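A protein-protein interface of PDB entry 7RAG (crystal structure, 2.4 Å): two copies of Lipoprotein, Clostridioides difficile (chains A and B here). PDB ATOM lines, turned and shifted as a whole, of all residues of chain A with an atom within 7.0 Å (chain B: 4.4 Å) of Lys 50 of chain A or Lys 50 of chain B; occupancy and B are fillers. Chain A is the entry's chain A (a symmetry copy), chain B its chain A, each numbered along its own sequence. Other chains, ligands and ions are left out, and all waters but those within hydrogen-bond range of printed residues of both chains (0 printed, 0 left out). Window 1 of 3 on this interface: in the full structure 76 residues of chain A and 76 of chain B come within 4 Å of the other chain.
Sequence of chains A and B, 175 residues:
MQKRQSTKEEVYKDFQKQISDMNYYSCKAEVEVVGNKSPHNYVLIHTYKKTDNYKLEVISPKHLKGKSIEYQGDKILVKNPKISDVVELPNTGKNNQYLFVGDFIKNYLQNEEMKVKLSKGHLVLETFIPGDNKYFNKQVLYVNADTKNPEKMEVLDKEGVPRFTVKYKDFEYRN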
ATOM      1  N   ILE A  19      17.372 -34.452  35.109  1.00  0.00           N
ATOM      2  CA  ILE A  19      17.468 -34.240  33.668  1.00  0.00           C
ATOM      3  C   ILE A  19      16.802 -32.937  33.232  1.00  0.00           C
ATOM      4  O   ILE A  19      17.163 -32.393  32.179  1.00  0.00           O
ATOM      5  CB  ILE A  19      16.894 -35.415  32.862  1.00  0.00           C
ATOM      6  CG1 ILE A  19      15.418 -35.640  33.186  1.00  0.00           C
ATOM      7  CG2 ILE A  19      17.701 -36.666  33.120  1.00  0.00           C
ATOM      8  CD1 ILE A  19      14.764 -36.687  32.316  1.00  0.00           C
ATOM      9  N   SER A  20      15.860 -32.404  34.018  1.00  0.00           N
ATOM     10  CA  SER A  20      15.231 -31.143  33.645  1.00  0.00           C
ATOM     11  C   SER A  20      16.195 -29.970  33.786  1.00  0.00           C
ATOM     12  O   SER A  20      16.238 -29.089  32.921  1.00  0.00           O
ATOM     13  CB  SER A  20      13.980 -30.916  34.484  1.00  0.00           C
ATOM     14  OG  SER A  20      13.040 -30.148  33.755  1.00  0.00           O
ATOM     15  N   ASP A  21      16.974 -29.936  34.870  1.00  0.00           N
ATOM     16  CA  ASP A  21      17.921 -28.849  35.100  1.00  0.00           C
ATOM     17  C   ASP A  21      19.168 -28.965  34.246  1.00  0.00           C
ATOM     18  O   ASP A  21      19.967 -28.028  34.205  1.00  0.00           O
ATOM     19  CB  ASP A  21      18.318 -28.796  36.570  1.00  0.00           C
ATOM     20  CG  ASP A  21      17.122 -28.655  37.481  1.00  0.00           C
ATOM     21  OD1 ASP A  21      16.098 -28.096  37.020  1.00  0.00           O
ATOM     22  OD2 ASP A  21      17.194 -29.099  38.653  1.00  0.00           O
ATOM     23  N   MET A  22      19.357 -30.082  33.584  1.00  0.00           N
ATOM     24  CA  MET A  22      20.510 -30.302  32.747  1.00  0.00           C
ATOM     25  C   MET A  22      20.582 -29.203  31.699  1.00  0.00           C
ATOM     26  O   MET A  22      19.595 -28.931  31.040  1.00  0.00           O
ATOM     27  CB  MET A  22      20.382 -31.673  32.092  1.00  0.00           C
ATOM     28  CG  MET A  22      21.616 -32.517  32.061  1.00  0.00           C
ATOM     29  SD  MET A  22      21.081 -34.409  31.865  1.00  0.00           S
ATOM     30  CE  MET A  22      21.072 -34.911  33.771  1.00  0.00           C
ATOM     31  N   ASN A  23      21.730 -28.557  31.556  1.00  0.00           N
ATOM     32  CA  ASN A  23      21.955 -27.625  30.461  1.00  0.00           C
ATOM     33  C   ASN A  23      22.999 -28.138  29.487  1.00  0.00           C
ATOM     34  O   ASN A  23      23.161 -27.559  28.406  1.00  0.00           O
ATOM     35  CB  ASN A  23      22.395 -26.249  30.998  1.00  0.00           C
ATOM     36  CG  ASN A  23      21.257 -25.485  31.694  1.00  0.00           C
ATOM     37  OD1 ASN A  23      20.085 -25.555  31.283  1.00  0.00           O
ATOM     38  ND2 ASN A  23      21.603 -24.756  32.759  1.00  0.00           N
ATOM     39  N   TYR A  24      23.707 -29.199  29.853  1.00  0.00           N
ATOM     40  CA  TYR A  24      24.715 -29.825  29.020  1.00  0.00           C
ATOM     41  C   TYR A  24      24.857 -31.274  29.468  1.00  0.00           C
ATOM     42  O   TYR A  24      24.803 -31.569  30.660  1.00  0.00           O
ATOM     43  CB  TYR A  24      26.054 -29.097  29.140  1.00  0.00           C
ATOM     44  CG  TYR A  24      27.202 -29.852  28.523  1.00  0.00           C
ATOM     45  CD1 TYR A  24      27.568 -29.625  27.203  1.00  0.00           C
ATOM     46  CD2 TYR A  24      27.909 -30.810  29.250  1.00  0.00           C
ATOM     47  CE1 TYR A  24      28.615 -30.314  26.623  1.00  0.00           C
ATOM     48  CE2 TYR A  24      28.950 -31.513  28.681  1.00  0.00           C
ATOM     49  CZ  TYR A  24      29.302 -31.257  27.366  1.00  0.00           C
ATOM     50  OH  TYR A  24      30.350 -31.942  26.792  1.00  0.00           O
ATOM     51  N   TYR A  25      25.026 -32.177  28.513  1.00  0.00           N
ATOM     52  CA  TYR A  25      25.468 -33.511  28.879  1.00  0.00           C
ATOM     53  C   TYR A  25      26.273 -34.081  27.733  1.00  0.00           C
ATOM     54  O   TYR A  25      26.202 -33.614  26.596  1.00  0.00           O
ATOM     55  CB  TYR A  25      24.310 -34.441  29.300  1.00  0.00           C
ATOM     56  CG  TYR A  25      23.504 -35.137  28.224  1.00  0.00           C
ATOM     57  CD1 TYR A  25      22.162 -34.829  28.026  1.00  0.00           C
ATOM     58  CD2 TYR A  25      24.052 -36.153  27.452  1.00  0.00           C
ATOM     59  CE1 TYR A  25      21.406 -35.466  27.067  1.00  0.00           C
ATOM     60  CE2 TYR A  25      23.304 -36.790  26.489  1.00  0.00           C
ATOM     61  CZ  TYR A  25      21.980 -36.438  26.305  1.00  0.00           C
ATOM     62  OH  TYR A  25      21.240 -37.077  25.350  1.00  0.00           O
ATOM     63  N   TYR A  48      24.767 -32.814  24.269  1.00  0.00           N
ATOM     64  CA  TYR A  48      23.587 -31.981  24.421  1.00  0.00           C
ATOM     65  C   TYR A  48      23.989 -30.659  25.054  1.00  0.00           C
ATOM     66  O   TYR A  48      24.656 -30.646  26.094  1.00  0.00           O
ATOM     67  CB  TYR A  48      22.553 -32.684  25.288  1.00  0.00           C
ATOM     68  CG  TYR A  48      21.418 -31.823  25.784  1.00  0.00           C
ATOM     69  CD1 TYR A  48      20.357 -31.502  24.951  1.00  0.00           C
ATOM     70  CD2 TYR A  48      21.373 -31.378  27.102  1.00  0.00           C
ATOM     71  CE1 TYR A  48      19.286 -30.758  25.400  1.00  0.00           C
ATOM     72  CE2 TYR A  48      20.295 -30.618  27.566  1.00  0.00           C
ATOM     73  CZ  TYR A  48      19.253 -30.313  26.702  1.00  0.00           C
ATOM     74  OH  TYR A  48      18.176 -29.565  27.119  1.00  0.00           O
ATOM     75  N   LYS A  49      23.603 -29.554  24.423  1.00  0.00           N
ATOM     76  CA  LYS A  49      23.620 -28.246  25.063  1.00  0.00           C
ATOM     77  C   LYS A  49      22.255 -27.595  24.879  1.00  0.00           C
ATOM     78  O   LYS A  49      21.660 -27.675  23.805  1.00  0.00           O
ATOM     79  CB  LYS A  49      24.749 -27.339  24.512  1.00  0.00           C
ATOM     80  CG  LYS A  49      24.827 -27.204  23.000  1.00  0.00           C
ATOM     81  N   LYS A  50      21.734 -27.004  25.949  1.00  0.00           N
ATOM     82  CA  LYS A  50      20.550 -26.157  25.852  1.00  0.00           C
ATOM     83  C   LYS A  50      21.007 -24.776  25.396  1.00  0.00           C
ATOM     84  O   LYS A  50      21.943 -24.218  25.966  1.00  0.00           O
ATOM     85  CB  LYS A  50      19.833 -26.087  27.201  1.00  0.00           C
ATOM     86  CG  LYS A  50      18.324 -26.100  27.105  1.00  0.00           C
ATOM     87  CD  LYS A  50      17.658 -25.873  28.454  1.00  0.00           C
ATOM     88  CE  LYS A  50      17.694 -27.127  29.294  1.00  0.00           C
ATOM     89  NZ  LYS A  50      17.483 -26.832  30.745  1.00  0.00           N
ATOM     90  N   THR A  51      20.413 -24.254  24.327  1.00  0.00           N
ATOM     91  CA  THR A  51      20.941 -23.056  23.685  1.00  0.00           C
ATOM     92  C   THR A  51      19.854 -21.998  23.559  1.00  0.00           C
ATOM     93  O   THR A  51      18.657 -22.307  23.562  1.00  0.00           O
ATOM     94  CB  THR A  51      21.534 -23.344  22.286  1.00  0.00           C
ATOM     95  OG1 THR A  51      20.482 -23.509  21.335  1.00  0.00           O
ATOM     96  CG2 THR A  51      22.373 -24.603  22.301  1.00  0.00           C
ATOM     97  N   ASP A  52      20.290 -20.744  23.465  1.00  0.00           N
ATOM     98  CA  ASP A  52      19.379 -19.615  23.347  1.00  0.00           C
ATOM     99  C   ASP A  52      18.969 -19.396  21.896  1.00  0.00           C
ATOM    100  O   ASP A  52      19.760 -19.587  20.973  1.00  0.00           O
ATOM    101  CB  ASP A  52      20.031 -18.350  23.899  1.00  0.00           C
ATOM    102  CG  ASP A  52      20.346 -18.458  25.373  1.00  0.00           C
ATOM    103  OD1 ASP A  52      21.035 -17.563  25.891  1.00  0.00           O
ATOM    104  OD2 ASP A  52      19.921 -19.438  26.021  1.00  0.00           O
ATOM    105  N   ASN A  53      17.711 -19.029  21.695  1.00  0.00           N
ATOM    106  CA  ASN A  53      17.217 -18.651  20.375  1.00  0.00           C
ATOM    107  C   ASN A  53      16.443 -17.348  20.512  1.00  0.00           C
ATOM    108  O   ASN A  53      15.450 -17.285  21.245  1.00  0.00           O
ATOM    109  CB  ASN A  53      16.342 -19.749  19.758  1.00  0.00           C
ATOM    110  CG  ASN A  53      15.662 -19.306  18.461  1.00  0.00           C
ATOM    111  OD1 ASN A  53      14.640 -18.613  18.480  1.00  0.00           O
ATOM    112  ND2 ASN A  53      16.218 -19.717  17.334  1.00  0.00           N
ATOM    113  N   SER B  20      17.040 -16.202  34.868  1.00  0.00           N
ATOM    114  CA  SER B  20      17.777 -17.439  34.644  1.00  0.00           C
ATOM    115  C   SER B  20      16.840 -18.607  34.350  1.00  0.00           C
ATOM    116  O   SER B  20      17.115 -19.419  33.459  1.00  0.00           O
ATOM    117  CB  SER B  20      18.657 -17.747  35.849  1.00  0.00           C
ATOM    118  OG  SER B  20      19.803 -18.470  35.440  1.00  0.00           O
ATOM    119  N   MET B  22      13.949 -18.436  33.060  1.00  0.00           N
ATOM    120  CA  MET B  22      13.159 -18.138  31.892  1.00  0.00           C
ATOM    121  C   MET B  22      13.474 -19.153  30.805  1.00  0.00           C
ATOM    122  O   MET B  22      14.634 -19.387  30.515  1.00  0.00           O
ATOM    123  CB  MET B  22      13.490 -16.722  31.430  1.00  0.00           C
ATOM    124  CG  MET B  22      12.334 -15.861  31.031  1.00  0.00           C
ATOM    125  SD  MET B  22      12.877 -13.968  31.180  1.00  0.00           S
ATOM    126  CE  MET B  22      12.211 -13.612  33.000  1.00  0.00           C
ATOM    127  N   ASN B  23      12.458 -19.770  30.219  1.00  0.00           N
ATOM    128  CA  ASN B  23      12.644 -20.613  29.048  1.00  0.00           C
ATOM    129  C   ASN B  23      12.001 -20.014  27.812  1.00  0.00           C
ATOM    130  O   ASN B  23      12.237 -20.506  26.702  1.00  0.00           O
ATOM    131  CB  ASN B  23      12.063 -22.019  29.290  1.00  0.00           C
ATOM    132  CG  ASN B  23      12.896 -22.849  30.281  1.00  0.00           C
ATOM    133  OD1 ASN B  23      14.136 -22.765  30.314  1.00  0.00           O
ATOM    134  ND2 ASN B  23      12.208 -23.653  31.099  1.00  0.00           N
ATOM    135  N   TYR B  48      12.111 -14.930  22.676  1.00  0.00           N
ATOM    136  CA  TYR B  48      13.174 -15.789  23.169  1.00  0.00           C
ATOM    137  C   TYR B  48      12.594 -17.150  23.519  1.00  0.00           C
ATOM    138  O   TYR B  48      11.605 -17.232  24.255  1.00  0.00           O
ATOM    139  CB  TYR B  48      13.828 -15.169  24.393  1.00  0.00           C
ATOM    140  CG  TYR B  48      14.729 -16.080  25.189  1.00  0.00           C
ATOM    141  CD1 TYR B  48      16.020 -16.351  24.759  1.00  0.00           C
ATOM    142  CD2 TYR B  48      14.316 -16.623  26.401  1.00  0.00           C
ATOM    143  CE1 TYR B  48      16.875 -17.141  25.497  1.00  0.00           C
ATOM    144  CE2 TYR B  48      15.173 -17.432  27.154  1.00  0.00           C
ATOM    145  CZ  TYR B  48      16.456 -17.685  26.691  1.00  0.00           C
ATOM    146  OH  TYR B  48      17.328 -18.477  27.401  1.00  0.00           O
ATOM    147  N   LYS B  49      13.192 -18.208  22.980  1.00  0.00           N
ATOM    148  CA  LYS B  49      12.969 -19.561  23.473  1.00  0.00           C
ATOM    149  C   LYS B  49      14.320 -20.215  23.730  1.00  0.00           C
ATOM    150  O   LYS B  49      15.253 -20.062  22.942  1.00  0.00           O
ATOM    151  CB  LYS B  49      12.118 -20.408  22.494  1.00  0.00           C
ATOM    152  CG  LYS B  49      12.577 -20.427  21.045  1.00  0.00           C
ATOM    153  N   LYS B  50      14.442 -20.892  24.867  1.00  0.00           N
ATOM    154  CA  LYS B  50      15.596 -21.746  25.127  1.00  0.00           C
ATOM    155  C   LYS B  50      15.347 -23.082  24.437  1.00  0.00           C
ATOM    156  O   LYS B  50      14.278 -23.669  24.598  1.00  0.00           O
ATOM    157  CB  LYS B  50      15.796 -21.928  26.632  1.00  0.00           C
ATOM    158  CG  LYS B  50      17.243 -21.928  27.072  1.00  0.00           C
ATOM    159  CD  LYS B  50      17.396 -22.266  28.548  1.00  0.00           C
ATOM    160  CE  LYS B  50      17.051 -21.080  29.415  1.00  0.00           C
ATOM    161  NZ  LYS B  50      16.743 -21.487  30.821  1.00  0.00           N
ATOM    162  N   THR B  51      16.286 -23.529  23.606  1.00  0.00           N
ATOM    163  CA  THR B  51      16.033 -24.668  22.731  1.00  0.00           C
ATOM    164  C   THR B  51      17.109 -25.728  22.915  1.00  0.00           C
ATOM    165  O   THR B  51      18.225 -25.437  23.361  1.00  0.00           O
ATOM    166  CB  THR B  51      15.963 -24.267  21.240  1.00  0.00           C
ATOM    167  OG1 THR B  51      17.280 -24.044  20.733  1.00  0.00           O
ATOM    168  CG2 THR B  51      15.156 -23.000  21.055  1.00  0.00           C
ATOM    169  N   ASP B  52      16.751 -26.965  22.579  1.00  0.00           N
ATOM    170  CA  ASP B  52      17.661 -28.095  22.702  1.00  0.00           C
ATOM    171  C   ASP B  52      18.557 -28.208  21.476  1.00  0.00           C
ATOM    172  O   ASP B  52      18.137 -27.938  20.351  1.00  0.00           O
ATOM    173  CB  ASP B  52      16.874 -29.388  22.893  1.00  0.00           C
ATOM    174  CG  ASP B  52      16.061 -29.388  24.167  1.00  0.00           C
ATOM    175  OD1 ASP B  52      15.246 -30.310  24.341  1.00  0.00           O
ATOM    176  OD2 ASP B  52      16.218 -28.466  24.996  1.00  0.00           O
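Tyr 48 of chain A touches Asp 52 of chain B, and with the chains exchanged Asp 52 of chain A touches Tyr 48 of chain B.
Lys 49 of chain A touches Asp 52 of chain B, and with the chains exchanged Asp 52 of chain A touches Lys 49 of chain B.
Lys 50 of chain A touches its own counterpart, Lys 50 of chain B.
Lys 50 of chain A touches Asp 52 of chain B, and with the chains exchanged Asp 52 of chain A touches Lys 50 of chain B.
8 positions are printed for both chains.
Of the 13 pairs that touch across the chains among the printed residues, 10 have their exchanged pair printed and touching as well.
Of the 13 printed residues of chain A, 6 touch a printed residue of chain B.
Hydrophobic or aromatic side chains of chain A within 4 Å of the printed part of chain B: Tyr 48.
Hydrophobic or aromatic side chains of chain B within 4 Å of the printed part of chain A: Tyr 48.
Among the printed residues, 13 pairs touch across the chains.
Among the printed residues, no Asp or Glu carboxylate lies within 4 Å of a Lys or Arg side-chain nitrogen of the other chain.
O of Thr 51 of chain B is in hydrogen-bond range of N of Thr 51 of chain A (2.7 Å).
The side-chain hydroxyl (OH) of Tyr 48 of chain A is in hydrogen-bond range of the side-chain carboxylate (OD2) of Asp 52 of chain B (3.1 Å).
The side-chain hydroxyl (OH) of Tyr 48 of chain B is in hydrogen-bond range of the side-chain carboxylate (OD2) of Asp 52 of chain A.
The backbone NH of Asn 53 of chain A is in hydrogen-bond range of the backbone carbonyl oxygen of Lys 49 of chain B, at 2.9 Å.
The backbone carbonyl oxygen (O) of Tyr 25 of chain A lies within hydrogen-bond range of the backbone NH (N) of Tyr 48 of chain A (2.8 Å).
The backbone carbonyl oxygen (O) of Met 22 of chain A sits at hydrogen-bond distance from the side-chain amino group (NZ) of Lys 50 of chain A (3.0 Å).
O of Asn 23 of chain B sits at hydrogen-bond distance from N of Lys 50 of chain B, 2.9 Å away.
The side-chain amino group of Lys 50 of chain B sits at hydrogen-bond distance from the backbone carbonyl oxygen of Ser 20 of chain B (3.4 Å).
The backbone carbonyl oxygen (O) of Ser 20 of chain A is in hydrogen-bond range of the side-chain amino group (NZ) of Lys 50 of chain A, 3.4 Å away.
The backbone carbonyl oxygen (O) of Asn 23 of chain A sits at hydrogen-bond distance from the backbone NH (N) of Lys 50 of chain A (2.9 Å).
Lys 50 of chain A touches just these residues of chain B: Lys 50, Thr 51 and Asp 52.
Lys 50 of chain B touches just these residues of chain A: Lys 50 (3.6 Å), Thr 51 (3.5 Å) and Asp 52 (3.8 Å).
Of the printed residues of chain B, Tyr 48 of chain A touches Asp 52.
Printed residues of chain B within 4 Å of Lys 49 of chain A: Asp 52.
Of the printed residues of chain A, Tyr 48 of chain B touches Asp 52 and Asn 53.
The nearest printed residue of chain B that does not touch Lys 50 of chain A is Asn 23 of chain B (5.1 Å).
The nearest residue of chain A that does not touch Lys 50 of chain B is Asn 53 of chain A (4.9 Å).
The nearest printed residue of chain B that does not touch Thr 51 of chain A is Lys 49 of chain B (4.1 Å).
Among the printed residues, merely in contact across the chains: Lys 49 of chain A with Asp 52 of chain B (3.9 Å), Lys 50 of chain A with Lys 50 of chain B (3.6 Å), Lys 50 of chain A with Thr 51 of chain B (3.5 Å), Lys 50 of chain A with Asp 52 of chain B (3.8 Å), Thr 51 of chain A with Lys 50 of chain B (3.5 Å), Asp 52 of chain A with Lys 49 of chain B (3.9 Å), Asp 52 of chain A with Lys 50 of chain B (3.8 Å), Asn 53 of chain A with Tyr 48 of chain B (3.3 Å) and Asn 53 of chain A with Thr 51 of chain B (3.7 Å).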
